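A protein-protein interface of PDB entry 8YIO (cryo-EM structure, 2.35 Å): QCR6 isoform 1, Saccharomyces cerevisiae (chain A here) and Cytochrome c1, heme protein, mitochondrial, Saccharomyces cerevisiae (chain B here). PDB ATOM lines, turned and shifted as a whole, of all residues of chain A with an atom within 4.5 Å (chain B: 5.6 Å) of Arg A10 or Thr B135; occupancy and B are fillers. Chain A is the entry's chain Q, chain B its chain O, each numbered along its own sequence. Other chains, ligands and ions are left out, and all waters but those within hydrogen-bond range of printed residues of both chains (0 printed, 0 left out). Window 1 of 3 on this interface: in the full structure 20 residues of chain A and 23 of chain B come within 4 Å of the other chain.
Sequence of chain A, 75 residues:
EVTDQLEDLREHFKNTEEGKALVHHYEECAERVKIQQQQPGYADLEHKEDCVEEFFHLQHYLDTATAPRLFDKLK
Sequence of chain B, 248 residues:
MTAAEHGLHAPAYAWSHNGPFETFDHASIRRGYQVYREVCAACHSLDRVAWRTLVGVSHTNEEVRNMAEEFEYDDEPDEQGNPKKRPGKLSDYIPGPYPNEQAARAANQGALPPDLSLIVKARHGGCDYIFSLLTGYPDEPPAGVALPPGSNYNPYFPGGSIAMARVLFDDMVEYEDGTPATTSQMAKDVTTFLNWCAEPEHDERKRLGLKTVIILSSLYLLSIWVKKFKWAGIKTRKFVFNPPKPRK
The side-chain carboxylate (OD2) of Asp A63 sits at hydrogen-bond distance from the side-chain hydroxyl (OH) of Tyr B156 (3.0 Å).
The backbone NH (N) of Leu A6 sits close to the side-chain hydroxyl (OG) of Ser B184, 3.4 Å away.
O of Thr B135 sits at hydrogen-bond distance from NH1 of Arg A10, at 3.3 Å.
Arg A10 touches just one residue of chain B: Thr B135 (3.3 Å).
Of chain A, only Leu A6 and Arg A10 come within 4 Å of Thr B135.
Printed residues of chain A within 4 Å of Tyr B156: Asp A63.
Printed residues of chain A within 4 Å of Ser B184: Leu A6 (3.3 Å).
Of the printed residues of chain B, Leu A6 touches Thr B135 and Ser B184.
Printed residues of chain B within 4 Å of Asp A63: Tyr B156 (3.0 Å).
The nearest residue of chain B that does not touch Arg A10 is Tyr B156 (4.3 Å).
The nearest printed residue of chain A that does not touch Thr B135 is Glu A7 (7.2 Å).
Among the printed residues, pairs that only touch across the chains: Leu A6 with Thr B135 (3.8 Å).
OG1 of Thr B135 is in hydrogen-bond range of O of Phe B131 (2.8 Å).
Of the 12 printed residues of chain A, 3 touch a printed residue of chain B.
Along chain A the printed residues that touch a printed residue of chain B span positions 6 to 63.
Hydrophobic or aromatic side chains of chain B within 4 Å of the printed part of chain A: Tyr B156.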
ATOM      1  N   LEU A   6       8.814 -22.527 -25.380  1.00  0.00           N
ATOM      2  CA  LEU A   6       8.430 -21.120 -25.448  1.00  0.00           C
ATOM      3  C   LEU A   6       9.296 -20.257 -24.540  1.00  0.00           C
ATOM      4  O   LEU A   6       9.528 -19.082 -24.841  1.00  0.00           O
ATOM      5  CB  LEU A   6       6.952 -20.964 -25.085  1.00  0.00           C
ATOM      6  CG  LEU A   6       6.267 -19.619 -25.332  1.00  0.00           C
ATOM      7  CD1 LEU A   6       6.332 -19.243 -26.786  1.00  0.00           C
ATOM      8  CD2 LEU A   6       4.826 -19.671 -24.885  1.00  0.00           C
ATOM      9  N   GLU A   7       9.795 -20.822 -23.439  1.00  0.00           N
ATOM     10  CA  GLU A   7      10.650 -20.061 -22.536  1.00  0.00           C
ATOM     11  C   GLU A   7      12.053 -19.876 -23.102  1.00  0.00           C
ATOM     12  O   GLU A   7      12.718 -18.885 -22.784  1.00  0.00           O
ATOM     13  CB  GLU A   7      10.718 -20.752 -21.177  1.00  0.00           C
ATOM     14  CG  GLU A   7       9.508 -20.507 -20.299  1.00  0.00           C
ATOM     15  CD  GLU A   7       9.652 -19.264 -19.447  1.00  0.00           C
ATOM     16  OE1 GLU A   7       9.538 -18.148 -19.996  1.00  0.00           O
ATOM     17  OE2 GLU A   7       9.882 -19.404 -18.227  1.00  0.00           O
ATOM     18  N   ASP A   8      12.521 -20.817 -23.927  1.00  0.00           N
ATOM     19  CA  ASP A   8      13.838 -20.680 -24.539  1.00  0.00           C
ATOM     20  C   ASP A   8      13.844 -19.591 -25.603  1.00  0.00           C
ATOM     21  O   ASP A   8      14.796 -18.808 -25.693  1.00  0.00           O
ATOM     22  CB  ASP A   8      14.277 -22.007 -25.151  1.00  0.00           C
ATOM     23  CG  ASP A   8      14.509 -23.079 -24.112  1.00  0.00           C
ATOM     24  OD1 ASP A   8      14.933 -22.741 -22.987  1.00  0.00           O
ATOM     25  OD2 ASP A   8      14.268 -24.262 -24.427  1.00  0.00           O
ATOM     26  N   LEU A   9      12.793 -19.537 -26.424  1.00  0.00           N
ATOM     27  CA  LEU A   9      12.715 -18.546 -27.490  1.00  0.00           C
ATOM     28  C   LEU A   9      12.493 -17.142 -26.945  1.00  0.00           C
ATOM     29  O   LEU A   9      12.995 -16.172 -27.520  1.00  0.00           O
ATOM     30  CB  LEU A   9      11.595 -18.914 -28.463  1.00  0.00           C
ATOM     31  CG  LEU A   9      11.934 -19.858 -29.615  1.00  0.00           C
ATOM     32  CD1 LEU A   9      10.670 -20.371 -30.291  1.00  0.00           C
ATOM     33  CD2 LEU A   9      12.832 -19.168 -30.616  1.00  0.00           C
ATOM     34  N   ARG A  10      11.748 -17.015 -25.845  1.00  0.00           N
ATOM     35  CA  ARG A  10      11.481 -15.696 -25.281  1.00  0.00           C
ATOM     36  C   ARG A  10      12.716 -15.105 -24.610  1.00  0.00           C
ATOM     37  O   ARG A  10      12.891 -13.883 -24.615  1.00  0.00           O
ATOM     38  CB  ARG A  10      10.321 -15.774 -24.288  1.00  0.00           C
ATOM     39  CG  ARG A  10       8.943 -15.683 -24.930  1.00  0.00           C
ATOM     40  CD  ARG A  10       7.833 -15.976 -23.934  1.00  0.00           C
ATOM     41  NE  ARG A  10       6.517 -15.663 -24.485  1.00  0.00           N
ATOM     42  CZ  ARG A  10       5.363 -15.951 -23.892  1.00  0.00           C
ATOM     43  NH1 ARG A  10       5.349 -16.562 -22.716  1.00  0.00           N
ATOM     44  NH2 ARG A  10       4.219 -15.622 -24.473  1.00  0.00           N
ATOM     45  N   GLU A  11      13.580 -15.947 -24.036  1.00  0.00           N
ATOM     46  CA  GLU A  11      14.787 -15.442 -23.386  1.00  0.00           C
ATOM     47  C   GLU A  11      15.872 -15.099 -24.401  1.00  0.00           C
ATOM     48  O   GLU A  11      16.647 -14.160 -24.181  1.00  0.00           O
ATOM     49  CB  GLU A  11      15.296 -16.456 -22.354  1.00  0.00           C
ATOM     50  CG  GLU A  11      16.476 -15.963 -21.508  1.00  0.00           C
ATOM     51  CD  GLU A  11      16.132 -14.759 -20.641  1.00  0.00           C
ATOM     52  OE1 GLU A  11      14.977 -14.651 -20.176  1.00  0.00           O
ATOM     53  OE2 GLU A  11      17.014 -13.896 -20.452  1.00  0.00           O
ATOM     54  N   HIS A  12      15.934 -15.831 -25.518  1.00  0.00           N
ATOM     55  CA  HIS A  12      16.881 -15.494 -26.576  1.00  0.00           C
ATOM     56  C   HIS A  12      16.530 -14.165 -27.229  1.00  0.00           C
ATOM     57  O   HIS A  12      17.422 -13.372 -27.557  1.00  0.00           O
ATOM     58  CB  HIS A  12      16.914 -16.602 -27.628  1.00  0.00           C
ATOM     59  CG  HIS A  12      17.627 -16.218 -28.889  1.00  0.00           C
ATOM     60  ND1 HIS A  12      16.978 -15.689 -29.984  1.00  0.00           N
ATOM     61  CD2 HIS A  12      18.937 -16.282 -29.225  1.00  0.00           C
ATOM     62  CE1 HIS A  12      17.856 -15.444 -30.940  1.00  0.00           C
ATOM     63  NE2 HIS A  12      19.052 -15.797 -30.505  1.00  0.00           N
ATOM     64  N   PHE A  13      15.243 -13.899 -27.419  1.00  0.00           N
ATOM     65  CA  PHE A  13      14.821 -12.688 -28.107  1.00  0.00           C
ATOM     66  C   PHE A  13      14.682 -11.489 -27.180  1.00  0.00           C
ATOM     67  O   PHE A  13      14.298 -10.411 -27.642  1.00  0.00           O
ATOM     68  CB  PHE A  13      13.514 -12.936 -28.857  1.00  0.00           C
ATOM     69  CG  PHE A  13      13.715 -13.555 -30.205  1.00  0.00           C
ATOM     70  CD1 PHE A  13      14.253 -12.815 -31.244  1.00  0.00           C
ATOM     71  CD2 PHE A  13      13.394 -14.884 -30.428  1.00  0.00           C
ATOM     72  CE1 PHE A  13      14.453 -13.384 -32.484  1.00  0.00           C
ATOM     73  CE2 PHE A  13      13.589 -15.459 -31.663  1.00  0.00           C
ATOM     74  CZ  PHE A  13      14.118 -14.708 -32.693  1.00  0.00           C
ATOM     75  N   LYS A  14      14.984 -11.641 -25.898  1.00  0.00           N
ATOM     76  CA  LYS A  14      15.123 -10.501 -25.011  1.00  0.00           C
ATOM     77  C   LYS A  14      16.559 -10.005 -24.937  1.00  0.00           C
ATOM     78  O   LYS A  14      16.841  -9.087 -24.163  1.00  0.00           O
ATOM     79  CB  LYS A  14      14.606 -10.852 -23.612  1.00  0.00           C
ATOM     80  CG  LYS A  14      13.093 -10.759 -23.493  1.00  0.00           C
ATOM     81  CD  LYS A  14      12.622 -10.779 -22.050  1.00  0.00           C
ATOM     82  CE  LYS A  14      12.858 -12.133 -21.413  1.00  0.00           C
ATOM     83  NZ  LYS A  14      12.090 -12.302 -20.151  1.00  0.00           N
ATOM     84  N   LEU A  62       8.112  -9.551 -28.728  1.00  0.00           N
ATOM     85  CA  LEU A  62       8.465 -10.957 -28.569  1.00  0.00           C
ATOM     86  C   LEU A  62       7.469 -11.874 -29.268  1.00  0.00           C
ATOM     87  O   LEU A  62       7.825 -12.995 -29.641  1.00  0.00           O
ATOM     88  CB  LEU A  62       8.561 -11.311 -27.086  1.00  0.00           C
ATOM     89  CG  LEU A  62       9.642 -10.605 -26.263  1.00  0.00           C
ATOM     90  CD1 LEU A  62       9.455 -10.867 -24.778  1.00  0.00           C
ATOM     91  CD2 LEU A  62      11.031 -11.028 -26.706  1.00  0.00           C
ATOM     92  N   ASP A  63       6.233 -11.416 -29.476  1.00  0.00           N
ATOM     93  CA  ASP A  63       5.230 -12.254 -30.120  1.00  0.00           C
ATOM     94  C   ASP A  63       5.413 -12.327 -31.631  1.00  0.00           C
ATOM     95  O   ASP A  63       5.163 -13.379 -32.224  1.00  0.00           O
ATOM     96  CB  ASP A  63       3.828 -11.750 -29.783  1.00  0.00           C
ATOM     97  CG  ASP A  63       3.373 -12.184 -28.406  1.00  0.00           C
ATOM     98  OD1 ASP A  63       3.873 -13.214 -27.914  1.00  0.00           O
ATOM     99  OD2 ASP A  63       2.517 -11.496 -27.815  1.00  0.00           O
ATOM    100  N   THR A  66       8.579 -14.868 -32.028  1.00  0.00           N
ATOM    101  CA  THR A  66       8.500 -16.239 -31.541  1.00  0.00           C
ATOM    102  C   THR A  66       7.454 -17.065 -32.284  1.00  0.00           C
ATOM    103  O   THR A  66       7.703 -18.233 -32.599  1.00  0.00           O
ATOM    104  CB  THR A  66       8.191 -16.229 -30.041  1.00  0.00           C
ATOM    105  OG1 THR A  66       9.160 -15.421 -29.365  1.00  0.00           O
ATOM    106  CG2 THR A  66       8.254 -17.617 -29.468  1.00  0.00           C
ATOM    107  N   TYR B  13      -0.015 -18.410 -35.084  1.00  0.00           N
ATOM    108  CA  TYR B  13       0.839 -19.586 -35.058  1.00  0.00           C
ATOM    109  C   TYR B  13       0.531 -20.477 -36.254  1.00  0.00           C
ATOM    110  O   TYR B  13      -0.527 -20.374 -36.880  1.00  0.00           O
ATOM    111  CB  TYR B  13       0.659 -20.374 -33.757  1.00  0.00           C
ATOM    112  CG  TYR B  13       1.131 -19.642 -32.524  1.00  0.00           C
ATOM    113  CD1 TYR B  13       2.451 -19.725 -32.106  1.00  0.00           C
ATOM    114  CD2 TYR B  13       0.253 -18.868 -31.777  1.00  0.00           C
ATOM    115  CE1 TYR B  13       2.883 -19.060 -30.978  1.00  0.00           C
ATOM    116  CE2 TYR B  13       0.678 -18.197 -30.651  1.00  0.00           C
ATOM    117  CZ  TYR B  13       1.991 -18.295 -30.258  1.00  0.00           C
ATOM    118  OH  TYR B  13       2.415 -17.628 -29.134  1.00  0.00           O
ATOM    119  N   ILE B 130      -6.836 -19.015 -27.328  1.00  0.00           N
ATOM    120  CA  ILE B 130      -6.850 -20.032 -26.277  1.00  0.00           C
ATOM    121  C   ILE B 130      -5.429 -20.462 -25.927  1.00  0.00           C
ATOM    122  O   ILE B 130      -5.102 -20.666 -24.754  1.00  0.00           O
ATOM    123  CB  ILE B 130      -7.718 -21.231 -26.710  1.00  0.00           C
ATOM    124  CG1 ILE B 130      -9.110 -20.765 -27.143  1.00  0.00           C
ATOM    125  CG2 ILE B 130      -7.824 -22.270 -25.603  1.00  0.00           C
ATOM    126  CD1 ILE B 130      -9.957 -20.207 -26.028  1.00  0.00           C
ATOM    127  N   PHE B 131      -4.560 -20.570 -26.932  1.00  0.00           N
ATOM    128  CA  PHE B 131      -3.171 -20.949 -26.690  1.00  0.00           C
ATOM    129  C   PHE B 131      -2.399 -19.842 -25.977  1.00  0.00           C
ATOM    130  O   PHE B 131      -1.571 -20.125 -25.107  1.00  0.00           O
ATOM    131  CB  PHE B 131      -2.492 -21.311 -28.012  1.00  0.00           C
ATOM    132  CG  PHE B 131      -1.070 -21.767 -27.859  1.00  0.00           C
ATOM    133  CD1 PHE B 131      -0.786 -23.059 -27.446  1.00  0.00           C
ATOM    134  CD2 PHE B 131      -0.016 -20.911 -28.137  1.00  0.00           C
ATOM    135  CE1 PHE B 131       0.519 -23.483 -27.305  1.00  0.00           C
ATOM    136  CE2 PHE B 131       1.292 -21.330 -27.993  1.00  0.00           C
ATOM    137  CZ  PHE B 131       1.558 -22.619 -27.578  1.00  0.00           C
ATOM    138  N   SER B 132      -2.650 -18.580 -26.336  1.00  0.00           N
ATOM    139  CA  SER B 132      -1.902 -17.480 -25.735  1.00  0.00           C
ATOM    140  C   SER B 132      -2.347 -17.208 -24.307  1.00  0.00           C
ATOM    141  O   SER B 132      -1.560 -16.699 -23.503  1.00  0.00           O
ATOM    142  CB  SER B 132      -2.045 -16.213 -26.574  1.00  0.00           C
ATOM    143  OG  SER B 132      -1.474 -16.382 -27.856  1.00  0.00           O
ATOM    144  N   LEU B 133      -3.598 -17.533 -23.977  1.00  0.00           N
ATOM    145  CA  LEU B 133      -4.083 -17.354 -22.613  1.00  0.00           C
ATOM    146  C   LEU B 133      -3.429 -18.344 -21.657  1.00  0.00           C
ATOM    147  O   LEU B 133      -3.053 -17.975 -20.540  1.00  0.00           O
ATOM    148  CB  LEU B 133      -5.603 -17.500 -22.581  1.00  0.00           C
ATOM    149  CG  LEU B 133      -6.323 -17.213 -21.265  1.00  0.00           C
ATOM    150  CD1 LEU B 133      -6.409 -15.719 -21.014  1.00  0.00           C
ATOM    151  CD2 LEU B 133      -7.707 -17.838 -21.270  1.00  0.00           C
ATOM    152  N   LEU B 134      -3.272 -19.599 -22.084  1.00  0.00           N
ATOM    153  CA  LEU B 134      -2.753 -20.635 -21.197  1.00  0.00           C
ATOM    154  C   LEU B 134      -1.261 -20.483 -20.941  1.00  0.00           C
ATOM    155  O   LEU B 134      -0.794 -20.780 -19.838  1.00  0.00           O
ATOM    156  CB  LEU B 134      -3.042 -22.015 -21.782  1.00  0.00           C
ATOM    157  CG  LEU B 134      -4.517 -22.395 -21.866  1.00  0.00           C
ATOM    158  CD1 LEU B 134      -4.711 -23.609 -22.753  1.00  0.00           C
ATOM    159  CD2 LEU B 134      -5.065 -22.634 -20.475  1.00  0.00           C
ATOM    160  N   THR B 135      -0.500 -20.030 -21.934  1.00  0.00           N
ATOM    161  CA  THR B 135       0.944 -19.893 -21.812  1.00  0.00           C
ATOM    162  C   THR B 135       1.380 -18.454 -21.560  1.00  0.00           C
ATOM    163  O   THR B 135       2.546 -18.120 -21.785  1.00  0.00           O
ATOM    164  CB  THR B 135       1.633 -20.431 -23.066  1.00  0.00           C
ATOM    165  OG1 THR B 135       1.104 -19.775 -24.222  1.00  0.00           O
ATOM    166  CG2 THR B 135       1.413 -21.919 -23.200  1.00  0.00           C
ATOM    167  N   GLY B 136       0.478 -17.599 -21.091  1.00  0.00           N
ATOM    168  CA  GLY B 136       0.784 -16.187 -20.997  1.00  0.00           C
ATOM    169  C   GLY B 136       0.664 -15.574 -19.619  1.00  0.00           C
ATOM    170  O   GLY B 136       0.470 -14.364 -19.499  1.00  0.00           O
ATOM    171  N   TYR B 137       0.774 -16.384 -18.577  1.00  0.00           N
ATOM    172  CA  TYR B 137       0.754 -15.862 -17.215  1.00  0.00           C
ATOM    173  C   TYR B 137       2.147 -15.374 -16.835  1.00  0.00           C
ATOM    174  O   TYR B 137       3.096 -16.164 -16.863  1.00  0.00           O
ATOM    175  CB  TYR B 137       0.301 -16.933 -16.230  1.00  0.00           C
ATOM    176  CG  TYR B 137      -1.184 -17.200 -16.216  1.00  0.00           C
ATOM    177  CD1 TYR B 137      -2.030 -16.478 -15.389  1.00  0.00           C
ATOM    178  CD2 TYR B 137      -1.736 -18.190 -17.020  1.00  0.00           C
ATOM    179  CE1 TYR B 137      -3.387 -16.723 -15.368  1.00  0.00           C
ATOM    180  CE2 TYR B 137      -3.089 -18.446 -17.004  1.00  0.00           C
ATOM    181  CZ  TYR B 137      -3.909 -17.711 -16.178  1.00  0.00           C
ATOM    182  OH  TYR B 137      -5.256 -17.964 -16.166  1.00  0.00           O
ATOM    183  N   TYR B 156      -3.729 -11.132 -21.911  1.00  0.00           N
ATOM    184  CA  TYR B 156      -4.610 -11.420 -23.036  1.00  0.00           C
ATOM    185  C   TYR B 156      -6.084 -11.401 -22.657  1.00  0.00           C
ATOM    186  O   TYR B 156      -6.935 -11.382 -23.551  1.00  0.00           O
ATOM    187  CB  TYR B 156      -4.253 -12.774 -23.654  1.00  0.00           C
ATOM    188  CG  TYR B 156      -2.840 -12.845 -24.183  1.00  0.00           C
ATOM    189  CD1 TYR B 156      -2.528 -12.359 -25.445  1.00  0.00           C
ATOM    190  CD2 TYR B 156      -1.819 -13.391 -23.418  1.00  0.00           C
ATOM    191  CE1 TYR B 156      -1.239 -12.417 -25.932  1.00  0.00           C
ATOM    192  CE2 TYR B 156      -0.526 -13.453 -23.897  1.00  0.00           C
ATOM    193  CZ  TYR B 156      -0.243 -12.963 -25.151  1.00  0.00           C
ATOM    194  OH  TYR B 156       1.041 -13.025 -25.630  1.00  0.00           O
ATOM    195  N   THR B 183       5.099 -27.275 -21.031  1.00  0.00           N
ATOM    196  CA  THR B 183       3.941 -26.388 -20.966  1.00  0.00           C
ATOM    197  C   THR B 183       3.426 -26.044 -22.358  1.00  0.00           C
ATOM    198  O   THR B 183       2.211 -25.981 -22.578  1.00  0.00           O
ATOM    199  CB  THR B 183       4.307 -25.119 -20.195  1.00  0.00           C
ATOM    200  OG1 THR B 183       4.960 -25.479 -18.974  1.00  0.00           O
ATOM    201  CG2 THR B 183       3.069 -24.300 -19.872  1.00  0.00           C
ATOM    202  N   SER B 184       4.334 -25.844 -23.313  1.00  0.00           N
ATOM    203  CA  SER B 184       3.934 -25.473 -24.665  1.00  0.00           C
ATOM    204  C   SER B 184       3.334 -26.646 -25.424  1.00  0.00           C
ATOM    205  O   SER B 184       2.488 -26.445 -26.301  1.00  0.00           O
ATOM    206  CB  SER B 184       5.135 -24.925 -25.422  1.00  0.00           C
ATOM    207  OG  SER B 184       5.869 -24.041 -24.605  1.00  0.00           O
ATOM    208  N   ALA B 187      -0.393 -27.279 -23.990  1.00  0.00           N
ATOM    209  CA  ALA B 187      -1.336 -26.247 -24.404  1.00  0.00           C
ATOM    210  C   ALA B 187      -1.694 -26.372 -25.877  1.00  0.00           C
ATOM    211  O   ALA B 187      -2.814 -26.032 -26.271  1.00  0.00           O
ATOM    212  CB  ALA B 187      -0.764 -24.862 -24.113  1.00  0.00           C
